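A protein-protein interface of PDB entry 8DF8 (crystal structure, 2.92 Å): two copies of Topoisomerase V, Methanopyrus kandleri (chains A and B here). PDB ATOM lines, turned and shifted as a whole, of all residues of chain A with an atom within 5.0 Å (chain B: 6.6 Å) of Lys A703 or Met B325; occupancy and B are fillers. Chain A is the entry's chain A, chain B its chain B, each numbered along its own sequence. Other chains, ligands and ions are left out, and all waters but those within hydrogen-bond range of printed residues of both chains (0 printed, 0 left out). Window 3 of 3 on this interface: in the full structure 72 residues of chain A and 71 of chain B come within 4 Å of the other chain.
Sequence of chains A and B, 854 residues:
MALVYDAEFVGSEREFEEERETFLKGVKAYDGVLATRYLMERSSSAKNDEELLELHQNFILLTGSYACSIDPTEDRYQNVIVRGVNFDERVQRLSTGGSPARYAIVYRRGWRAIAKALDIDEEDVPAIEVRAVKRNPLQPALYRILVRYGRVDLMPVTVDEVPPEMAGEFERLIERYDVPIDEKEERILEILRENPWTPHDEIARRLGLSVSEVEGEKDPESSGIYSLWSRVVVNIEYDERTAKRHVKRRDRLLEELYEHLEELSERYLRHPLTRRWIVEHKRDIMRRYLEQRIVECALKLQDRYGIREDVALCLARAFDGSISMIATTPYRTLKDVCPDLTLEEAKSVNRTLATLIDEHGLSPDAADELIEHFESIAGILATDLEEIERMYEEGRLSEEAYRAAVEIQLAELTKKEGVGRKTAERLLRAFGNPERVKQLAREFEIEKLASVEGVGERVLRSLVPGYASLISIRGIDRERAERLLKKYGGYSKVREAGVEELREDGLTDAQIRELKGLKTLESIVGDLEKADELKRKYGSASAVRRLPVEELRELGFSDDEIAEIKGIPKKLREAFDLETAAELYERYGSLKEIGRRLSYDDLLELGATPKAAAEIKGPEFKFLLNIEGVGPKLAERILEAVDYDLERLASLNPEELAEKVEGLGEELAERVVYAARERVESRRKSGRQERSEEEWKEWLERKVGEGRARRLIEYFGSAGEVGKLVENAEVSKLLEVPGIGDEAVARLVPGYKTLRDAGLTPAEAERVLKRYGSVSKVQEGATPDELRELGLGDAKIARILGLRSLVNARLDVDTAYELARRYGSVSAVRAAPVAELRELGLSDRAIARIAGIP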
ATOM      1  N   TRP A 699       0.420   6.603  -9.268  1.00  0.00           N
ATOM      2  CA  TRP A 699      -0.389   6.397 -10.465  1.00  0.00           C
ATOM      3  C   TRP A 699       0.470   5.920 -11.630  1.00  0.00           C
ATOM      4  O   TRP A 699       0.040   5.072 -12.422  1.00  0.00           O
ATOM      5  CB  TRP A 699      -1.124   7.686 -10.824  1.00  0.00           C
ATOM      6  CG  TRP A 699      -2.084   7.538 -11.958  1.00  0.00           C
ATOM      7  CD1 TRP A 699      -3.355   7.044 -11.898  1.00  0.00           C
ATOM      8  CD2 TRP A 699      -1.856   7.895 -13.326  1.00  0.00           C
ATOM      9  NE1 TRP A 699      -3.931   7.067 -13.145  1.00  0.00           N
ATOM     10  CE2 TRP A 699      -3.031   7.586 -14.039  1.00  0.00           C
ATOM     11  CE3 TRP A 699      -0.772   8.443 -14.016  1.00  0.00           C
ATOM     12  CZ2 TRP A 699      -3.152   7.807 -15.409  1.00  0.00           C
ATOM     13  CZ3 TRP A 699      -0.895   8.665 -15.376  1.00  0.00           C
ATOM     14  CH2 TRP A 699      -2.075   8.346 -16.058  1.00  0.00           C
ATOM     15  N   LEU A 700       1.691   6.444 -11.742  1.00  0.00           N
ATOM     16  CA  LEU A 700       2.606   5.974 -12.777  1.00  0.00           C
ATOM     17  C   LEU A 700       3.029   4.534 -12.515  1.00  0.00           C
ATOM     18  O   LEU A 700       3.010   3.696 -13.423  1.00  0.00           O
ATOM     19  CB  LEU A 700       3.827   6.889 -12.856  1.00  0.00           C
ATOM     20  CG  LEU A 700       3.590   8.264 -13.477  1.00  0.00           C
ATOM     21  CD1 LEU A 700       4.856   9.098 -13.409  1.00  0.00           C
ATOM     22  CD2 LEU A 700       3.111   8.120 -14.911  1.00  0.00           C
ATOM     23  N   GLU A 701       3.409   4.228 -11.270  1.00  0.00           N
ATOM     24  CA  GLU A 701       3.773   2.857 -10.923  1.00  0.00           C
ATOM     25  C   GLU A 701       2.631   1.889 -11.198  1.00  0.00           C
ATOM     26  O   GLU A 701       2.869   0.706 -11.470  1.00  0.00           O
ATOM     27  CB  GLU A 701       4.190   2.782  -9.455  1.00  0.00           C
ATOM     28  CG  GLU A 701       5.509   3.471  -9.147  1.00  0.00           C
ATOM     29  CD  GLU A 701       5.899   3.358  -7.685  1.00  0.00           C
ATOM     30  OE1 GLU A 701       5.073   2.875  -6.882  1.00  0.00           O
ATOM     31  OE2 GLU A 701       7.031   3.757  -7.340  1.00  0.00           O
ATOM     32  N   ARG A 702       1.389   2.369 -11.133  1.00  0.00           N
ATOM     33  CA  ARG A 702       0.254   1.536 -11.510  1.00  0.00           C
ATOM     34  C   ARG A 702       0.150   1.391 -13.025  1.00  0.00           C
ATOM     35  O   ARG A 702      -0.052   0.286 -13.539  1.00  0.00           O
ATOM     36  CB  ARG A 702      -1.044   2.118 -10.942  1.00  0.00           C
ATOM     37  CG  ARG A 702      -1.271   1.835  -9.467  1.00  0.00           C
ATOM     38  CD  ARG A 702      -2.630   2.349  -9.005  1.00  0.00           C
ATOM     39  NE  ARG A 702      -3.730   1.764  -9.767  1.00  0.00           N
ATOM     40  CZ  ARG A 702      -4.415   2.400 -10.709  1.00  0.00           C
ATOM     41  NH1 ARG A 702      -4.151   3.656 -11.027  1.00  0.00           N
ATOM     42  NH2 ARG A 702      -5.391   1.758 -11.346  1.00  0.00           N
ATOM     43  N   LYS A 703       0.283   2.497 -13.759  1.00  0.00           N
ATOM     44  CA  LYS A 703      -0.049   2.463 -15.179  1.00  0.00           C
ATOM     45  C   LYS A 703       1.072   1.905 -16.046  1.00  0.00           C
ATOM     46  O   LYS A 703       0.793   1.358 -17.116  1.00  0.00           O
ATOM     47  CB  LYS A 703      -0.443   3.860 -15.664  1.00  0.00           C
ATOM     48  CG  LYS A 703      -1.845   4.282 -15.236  1.00  0.00           C
ATOM     49  CD  LYS A 703      -2.908   3.325 -15.770  1.00  0.00           C
ATOM     50  CE  LYS A 703      -4.206   3.426 -14.973  1.00  0.00           C
ATOM     51  NZ  LYS A 703      -5.181   2.363 -15.354  1.00  0.00           N
ATOM     52  N   VAL A 704       2.330   2.045 -15.638  1.00  0.00           N
ATOM     53  CA  VAL A 704       3.414   1.559 -16.490  1.00  0.00           C
ATOM     54  C   VAL A 704       4.409   0.707 -15.706  1.00  0.00           C
ATOM     55  O   VAL A 704       5.444   0.284 -16.241  1.00  0.00           O
ATOM     56  CB  VAL A 704       4.131   2.730 -17.186  1.00  0.00           C
ATOM     57  CG1 VAL A 704       3.228   3.351 -18.240  1.00  0.00           C
ATOM     58  CG2 VAL A 704       4.570   3.758 -16.173  1.00  0.00           C
ATOM     59  N   GLY A 705       4.106   0.442 -14.442  1.00  0.00           N
ATOM     60  CA  GLY A 705       4.989  -0.365 -13.629  1.00  0.00           C
ATOM     61  C   GLY A 705       6.121   0.450 -13.026  1.00  0.00           C
ATOM     62  O   GLY A 705       6.464   1.537 -13.489  1.00  0.00           O
ATOM     63  N   ARG A 708       9.307   1.508 -15.515  1.00  0.00           N
ATOM     64  CA  ARG A 708       9.005   2.577 -16.460  1.00  0.00           C
ATOM     65  C   ARG A 708       8.568   3.849 -15.744  1.00  0.00           C
ATOM     66  O   ARG A 708       8.827   4.955 -16.237  1.00  0.00           O
ATOM     67  CB  ARG A 708       7.953   2.103 -17.462  1.00  0.00           C
ATOM     68  CG  ARG A 708       8.562   1.258 -18.569  1.00  0.00           C
ATOM     69  CD  ARG A 708       7.541   0.737 -19.559  1.00  0.00           C
ATOM     70  NE  ARG A 708       6.947  -0.518 -19.118  1.00  0.00           N
ATOM     71  CZ  ARG A 708       6.319  -1.366 -19.921  1.00  0.00           C
ATOM     72  NH1 ARG A 708       6.186  -1.120 -21.215  1.00  0.00           N
ATOM     73  NH2 ARG A 708       5.819  -2.490 -19.417  1.00  0.00           N
ATOM     74  N   GLU A 743       2.684   0.615 -26.095  1.00  0.00           N
ATOM     75  CA  GLU A 743       1.838  -0.060 -25.115  1.00  0.00           C
ATOM     76  C   GLU A 743       1.892   0.580 -23.735  1.00  0.00           C
ATOM     77  O   GLU A 743       1.030   0.278 -22.903  1.00  0.00           O
ATOM     78  CB  GLU A 743       2.214  -1.541 -25.017  1.00  0.00           C
ATOM     79  CG  GLU A 743       1.740  -2.383 -26.193  1.00  0.00           C
ATOM     80  CD  GLU A 743       0.242  -2.268 -26.427  1.00  0.00           C
ATOM     81  OE1 GLU A 743      -0.535  -2.633 -25.518  1.00  0.00           O
ATOM     82  OE2 GLU A 743      -0.160  -1.814 -27.520  1.00  0.00           O
ATOM     83  N   ALA A 744       2.866   1.452 -23.470  1.00  0.00           N
ATOM     84  CA  ALA A 744       2.897   2.196 -22.216  1.00  0.00           C
ATOM     85  C   ALA A 744       2.195   3.544 -22.331  1.00  0.00           C
ATOM     86  O   ALA A 744       1.470   3.948 -21.414  1.00  0.00           O
ATOM     87  CB  ALA A 744       4.344   2.399 -21.758  1.00  0.00           C
ATOM     88  N   ARG A 747      -1.463   3.100 -22.339  1.00  0.00           N
ATOM     89  CA  ARG A 747      -1.955   2.884 -20.987  1.00  0.00           C
ATOM     90  C   ARG A 747      -1.850   4.142 -20.133  1.00  0.00           C
ATOM     91  O   ARG A 747      -2.499   4.222 -19.083  1.00  0.00           O
ATOM     92  CB  ARG A 747      -1.200   1.719 -20.340  1.00  0.00           C
ATOM     93  CG  ARG A 747      -1.843   1.203 -19.064  1.00  0.00           C
ATOM     94  CD  ARG A 747      -1.389  -0.202 -18.721  1.00  0.00           C
ATOM     95  NE  ARG A 747      -1.666  -0.522 -17.326  1.00  0.00           N
ATOM     96  CZ  ARG A 747      -2.840  -0.944 -16.876  1.00  0.00           C
ATOM     97  NH1 ARG A 747      -3.871  -1.114 -17.687  1.00  0.00           N
ATOM     98  NH2 ARG A 747      -2.982  -1.200 -15.578  1.00  0.00           N
ATOM     99  N   LEU A 748      -1.068   5.129 -20.569  1.00  0.00           N
ATOM    100  CA  LEU A 748      -1.015   6.422 -19.894  1.00  0.00           C
ATOM    101  C   LEU A 748      -2.029   7.409 -20.465  1.00  0.00           C
ATOM    102  O   LEU A 748      -2.772   8.044 -19.710  1.00  0.00           O
ATOM    103  CB  LEU A 748       0.394   7.015 -19.990  1.00  0.00           C
ATOM    104  CG  LEU A 748       1.450   6.469 -19.031  1.00  0.00           C
ATOM    105  CD1 LEU A 748       2.796   7.123 -19.291  1.00  0.00           C
ATOM    106  CD2 LEU A 748       1.017   6.689 -17.594  1.00  0.00           C
ATOM    107  N   ARG B 293      -9.206  -7.372  -9.866  1.00  0.00           N
ATOM    108  CA  ARG B 293      -8.481  -7.423 -11.130  1.00  0.00           C
ATOM    109  C   ARG B 293      -7.124  -8.099 -10.964  1.00  0.00           C
ATOM    110  O   ARG B 293      -6.677  -8.835 -11.852  1.00  0.00           O
ATOM    111  CB  ARG B 293      -8.328  -6.010 -11.696  1.00  0.00           C
ATOM    112  CG  ARG B 293      -6.962  -5.703 -12.289  1.00  0.00           C
ATOM    113  CD  ARG B 293      -6.996  -4.424 -13.111  1.00  0.00           C
ATOM    114  NE  ARG B 293      -7.764  -3.369 -12.458  1.00  0.00           N
ATOM    115  CZ  ARG B 293      -7.252  -2.471 -11.629  1.00  0.00           C
ATOM    116  NH1 ARG B 293      -5.965  -2.470 -11.318  1.00  0.00           N
ATOM    117  NH2 ARG B 293      -8.049  -1.547 -11.101  1.00  0.00           N
ATOM    118  N   PHE B 319       2.264  -5.051 -11.469  1.00  0.00           N
ATOM    119  CA  PHE B 319       1.956  -4.456 -12.762  1.00  0.00           C
ATOM    120  C   PHE B 319       0.466  -4.166 -12.911  1.00  0.00           C
ATOM    121  O   PHE B 319      -0.063  -4.183 -14.029  1.00  0.00           O
ATOM    122  CB  PHE B 319       2.439  -5.351 -13.904  1.00  0.00           C
ATOM    123  CG  PHE B 319       3.934  -5.406 -14.031  1.00  0.00           C
ATOM    124  CD1 PHE B 319       4.675  -6.320 -13.299  1.00  0.00           C
ATOM    125  CD2 PHE B 319       4.600  -4.539 -14.879  1.00  0.00           C
ATOM    126  CE1 PHE B 319       6.053  -6.370 -13.414  1.00  0.00           C
ATOM    127  CE2 PHE B 319       5.976  -4.581 -14.998  1.00  0.00           C
ATOM    128  CZ  PHE B 319       6.704  -5.499 -14.267  1.00  0.00           C
ATOM    129  N   ASP B 320      -0.222  -3.902 -11.797  1.00  0.00           N
ATOM    130  CA  ASP B 320      -1.624  -3.476 -11.802  1.00  0.00           C
ATOM    131  C   ASP B 320      -2.526  -4.478 -12.524  1.00  0.00           C
ATOM    132  O   ASP B 320      -3.577  -4.114 -13.056  1.00  0.00           O
ATOM    133  CB  ASP B 320      -1.767  -2.078 -12.414  1.00  0.00           C
ATOM    134  CG  ASP B 320      -3.073  -1.402 -12.042  1.00  0.00           C
ATOM    135  OD1 ASP B 320      -3.285  -1.138 -10.838  1.00  0.00           O
ATOM    136  OD2 ASP B 320      -3.882  -1.126 -12.953  1.00  0.00           O
ATOM    137  N   SER B 322      -2.069  -6.065 -15.353  1.00  0.00           N
ATOM    138  CA  SER B 322      -2.102  -5.850 -16.796  1.00  0.00           C
ATOM    139  C   SER B 322      -1.219  -6.892 -17.473  1.00  0.00           C
ATOM    140  O   SER B 322       0.012  -6.813 -17.396  1.00  0.00           O
ATOM    141  CB  SER B 322      -1.643  -4.438 -17.149  1.00  0.00           C
ATOM    142  OG  SER B 322      -1.607  -4.263 -18.555  1.00  0.00           O
ATOM    143  N   ILE B 323      -1.850  -7.858 -18.144  1.00  0.00           N
ATOM    144  CA  ILE B 323      -1.093  -8.862 -18.886  1.00  0.00           C
ATOM    145  C   ILE B 323      -0.319  -8.214 -20.025  1.00  0.00           C
ATOM    146  O   ILE B 323       0.851  -8.537 -20.265  1.00  0.00           O
ATOM    147  CB  ILE B 323      -2.034  -9.970 -19.396  1.00  0.00           C
ATOM    148  CG1 ILE B 323      -2.421 -10.909 -18.252  1.00  0.00           C
ATOM    149  CG2 ILE B 323      -1.392 -10.745 -20.538  1.00  0.00           C
ATOM    150  CD1 ILE B 323      -3.333 -12.037 -18.677  1.00  0.00           C
ATOM    151  N   SER B 324      -0.955  -7.277 -20.736  1.00  0.00           N
ATOM    152  CA  SER B 324      -0.301  -6.612 -21.859  1.00  0.00           C
ATOM    153  C   SER B 324       0.933  -5.835 -21.431  1.00  0.00           C
ATOM    154  O   SER B 324       1.793  -5.543 -22.271  1.00  0.00           O
ATOM    155  CB  SER B 324      -1.284  -5.674 -22.561  1.00  0.00           C
ATOM    156  OG  SER B 324      -1.783  -4.695 -21.666  1.00  0.00           O
ATOM    157  N   MET B 325       1.044  -5.495 -20.149  1.00  0.00           N
ATOM    158  CA  MET B 325       2.197  -4.755 -19.654  1.00  0.00           C
ATOM    159  C   MET B 325       3.321  -5.677 -19.201  1.00  0.00           C
ATOM    160  O   MET B 325       4.497  -5.381 -19.439  1.00  0.00           O
ATOM    161  CB  MET B 325       1.782  -3.835 -18.503  1.00  0.00           C
ATOM    162  CG  MET B 325       2.464  -2.473 -18.511  1.00  0.00           C
ATOM    163  SD  MET B 325       1.818  -1.360 -19.780  1.00  0.00           S
ATOM    164  CE  MET B 325       2.938  -1.659 -21.144  1.00  0.00           C
ATOM    165  N   ILE B 326       2.980  -6.794 -18.549  1.00  0.00           N
ATOM    166  CA  ILE B 326       3.997  -7.761 -18.150  1.00  0.00           C
ATOM    167  C   ILE B 326       4.681  -8.341 -19.377  1.00  0.00           C
ATOM    168  O   ILE B 326       5.883  -8.635 -19.349  1.00  0.00           O
ATOM    169  CB  ILE B 326       3.367  -8.862 -17.273  1.00  0.00           C
ATOM    170  CG1 ILE B 326       2.668  -8.243 -16.062  1.00  0.00           C
ATOM    171  CG2 ILE B 326       4.418  -9.860 -16.819  1.00  0.00           C
ATOM    172  CD1 ILE B 326       1.954  -9.249 -15.187  1.00  0.00           C
ATOM    173  N   ALA B 327       3.942  -8.490 -20.478  1.00  0.00           N
ATOM    174  CA  ALA B 327       4.493  -9.034 -21.712  1.00  0.00           C
ATOM    175  C   ALA B 327       5.449  -8.077 -22.415  1.00  0.00           C
ATOM    176  O   ALA B 327       6.064  -8.472 -23.412  1.00  0.00           O
ATOM    177  CB  ALA B 327       3.359  -9.420 -22.663  1.00  0.00           C
ATOM    178  N   THR B 328       5.589  -6.840 -21.934  1.00  0.00           N
ATOM    179  CA  THR B 328       6.521  -5.884 -22.522  1.00  0.00           C
ATOM    180  C   THR B 328       7.584  -5.422 -21.533  1.00  0.00           C
ATOM    181  O   THR B 328       8.292  -4.447 -21.812  1.00  0.00           O
ATOM    182  CB  THR B 328       5.767  -4.668 -23.071  1.00  0.00           C
ATOM    183  OG1 THR B 328       4.928  -4.124 -22.045  1.00  0.00           O
ATOM    184  CG2 THR B 328       4.911  -5.064 -24.262  1.00  0.00           C
ATOM    185  N   THR B 329       7.718  -6.098 -20.395  1.00  0.00           N
ATOM    186  CA  THR B 329       8.693  -5.762 -19.364  1.00  0.00           C
ATOM    187  C   THR B 329       9.914  -6.659 -19.486  1.00  0.00           C
ATOM    188  O   THR B 329       9.764  -7.886 -19.570  1.00  0.00           O
ATOM    189  CB  THR B 329       8.071  -5.916 -17.980  1.00  0.00           C
ATOM    190  OG1 THR B 329       7.013  -4.962 -17.828  1.00  0.00           O
ATOM    191  CG2 THR B 329       9.108  -5.690 -16.895  1.00  0.00           C
ATOM    192  N   LEU B 334      11.498  -8.006 -14.194  1.00  0.00           N
ATOM    193  CA  LEU B 334      10.626  -9.045 -13.657  1.00  0.00           C
ATOM    194  C   LEU B 334      11.307  -9.805 -12.527  1.00  0.00           C
ATOM    195  O   LEU B 334      10.667 -10.151 -11.528  1.00  0.00           O
ATOM    196  CB  LEU B 334      10.200 -10.001 -14.771  1.00  0.00           C
ATOM    197  CG  LEU B 334       9.400  -9.401 -15.929  1.00  0.00           C
ATOM    198  CD1 LEU B 334       9.219 -10.414 -17.050  1.00  0.00           C
ATOM    199  CD2 LEU B 334       8.052  -8.908 -15.434  1.00  0.00           C
ATOM    200  N   ASN B 350       6.137 -13.340 -21.332  1.00  0.00           N
ATOM    201  CA  ASN B 350       6.645 -12.373 -22.305  1.00  0.00           C
ATOM    202  C   ASN B 350       6.986 -13.126 -23.583  1.00  0.00           C
ATOM    203  O   ASN B 350       8.060 -13.720 -23.701  1.00  0.00           O
ATOM    204  CB  ASN B 350       7.857 -11.631 -21.752  1.00  0.00           C
ATOM    205  CG  ASN B 350       8.268 -10.449 -22.618  1.00  0.00           C
ATOM    206  OD1 ASN B 350       8.192 -10.499 -23.848  1.00  0.00           O
ATOM    207  ND2 ASN B 350       8.710  -9.374 -21.974  1.00  0.00           N
ATOM    208  N   GLU B 375      10.074  -2.524 -26.919  1.00  0.00           N
ATOM    209  CA  GLU B 375       8.884  -3.036 -26.239  1.00  0.00           C
ATOM    210  C   GLU B 375       8.451  -4.423 -26.704  1.00  0.00           C
ATOM    211  O   GLU B 375       8.312  -5.334 -25.880  1.00  0.00           O
ATOM    212  CB  GLU B 375       7.709  -2.065 -26.383  1.00  0.00           C
ATOM    213  CG  GLU B 375       6.913  -1.896 -25.102  1.00  0.00           C
ATOM    214  CD  GLU B 375       6.057  -0.650 -25.101  1.00  0.00           C
ATOM    215  OE1 GLU B 375       5.368  -0.405 -26.116  1.00  0.00           O
ATOM    216  OE2 GLU B 375       6.072   0.081 -24.087  1.00  0.00           O
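NH2 of Arg A708 sits at hydrogen-bond distance from OG1 of Thr B329, 3.2 Å away.
The guanidinium group (NH2) of Arg A747 lies within salt-bridge range of the side-chain carboxylate (OD2) of Asp B320, at 2.8 Å.
The backbone carbonyl oxygen (O) of Glu A743 lies close to the side-chain sulfur (SD) of Met B325.
O of Met B325 lies within hydrogen-bond range of NH2 of Arg A708, at 3.2 Å.
The side-chain hydroxyl (OG1) of Thr B328 lies within hydrogen-bond range of the guanidinium group (NH2) of Arg A708.
The guanidinium group of Arg A708 is in salt-bridge range of the side-chain carboxylate of Glu B375 (3.1 Å).
The side-chain carboxylate of Asp B320 lies within salt-bridge range of the guanidinium group of Arg A702 (3.1 Å).
OE1 of Glu B375 is in hydrogen-bond range of N of Glu A743 (2.9 Å).
The backbone carbonyl oxygen of Met B325 sits at hydrogen-bond distance from the side-chain hydroxyl of Thr B328 (2.9 Å).
The backbone carbonyl oxygen (O) of Thr B329 sits at hydrogen-bond distance from the side-chain amide nitrogen (ND2) of Asn B350 (3.0 Å).
The side-chain hydroxyl (OG) of Ser B322 lies within hydrogen-bond range of the side-chain hydroxyl (OG) of Ser B324 (3.1 Å).
O of Val A704 lies close to NE of Arg A708 (3.3 Å).
The backbone carbonyl oxygen (O) of Ser B324 is in hydrogen-bond range of the side-chain hydroxyl (OG1) of Thr B328 (3.4 Å).
The backbone carbonyl oxygen (O) of Met B325 sits at hydrogen-bond distance from the side-chain hydroxyl (OG1) of Thr B329 (3.0 Å).
Lys A703 touches Met B325.
Ala A744 touches Met B325 (N to CE, 3.9 Å).
Ala A744 touches Glu B375 (N to OE2, 3.5 Å).
Ser B322 touches Arg A747 (CB to CZ, 3.7 Å).
CD of Arg A747 touches SD of Met B325 (3.6 Å).
Printed residues of chain B within 4 Å of Lys A703: Met B325 (3.9 Å).
Printed residues of chain B within 4 Å of Arg A708: Met B325 (3.2 Å), Thr B328 (3.2 Å), Thr B329 (3.2 Å) and Glu B375 (3.1 Å).
Printed residues of chain B within 4 Å of Glu A743: Met B325 and Glu B375.
Of the printed residues of chain B, Ala A744 touches Met B325 (3.9 Å) and Glu B375 (3.5 Å).
Printed residues of chain B within 4 Å of Arg A747: Asp B320, Ser B322 and Met B325.
Arg B293 touches none of the printed residues of chain A.
Of the printed residues of chain A, Asp B320 touches Arg A702 (3.1 Å) and Arg A747 (2.8 Å).
Of the printed residues of chain A, Met B325 touches Lys A703 (3.9 Å), Arg A708 (3.2 Å), Glu A743 (3.2 Å), Ala A744 (3.9 Å) and Arg A747 (3.6 Å).
Leu B334 touches none of the printed residues of chain A.
The nearest printed residue of chain B that does not touch Lys A703 is Asp B320 (4.4 Å).
The nearest printed residue of chain A that does not touch Met B325 is Val A704 (4.6 Å).
Printed residues of chain B that touch a printed residue of chain A: Asp B320, Ser B322, Met B325, Thr B328, Thr B329 and Glu B375.
Hydrophobic or aromatic side chains of chain B within 4 Å of the printed part of chain A: Met B325.
Of the 12 printed residues of chain A, 6 touch a printed residue of chain B.
Among the printed residues, 13 pairs touch across the chains.
Among the printed residues, Asp or Glu carboxylates within 4 Å of a Lys or Arg side-chain nitrogen of the other chain: Arg A702 with Asp B320 (3.1 Å), Arg A708 with Glu B375 (3.1 Å) and Arg A747 with Asp B320 (2.8 Å).
No position is printed for both chains.
Of the 13 pairs that touch across the chains among the printed residues, none has its exchanged pair printed and touching as well.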
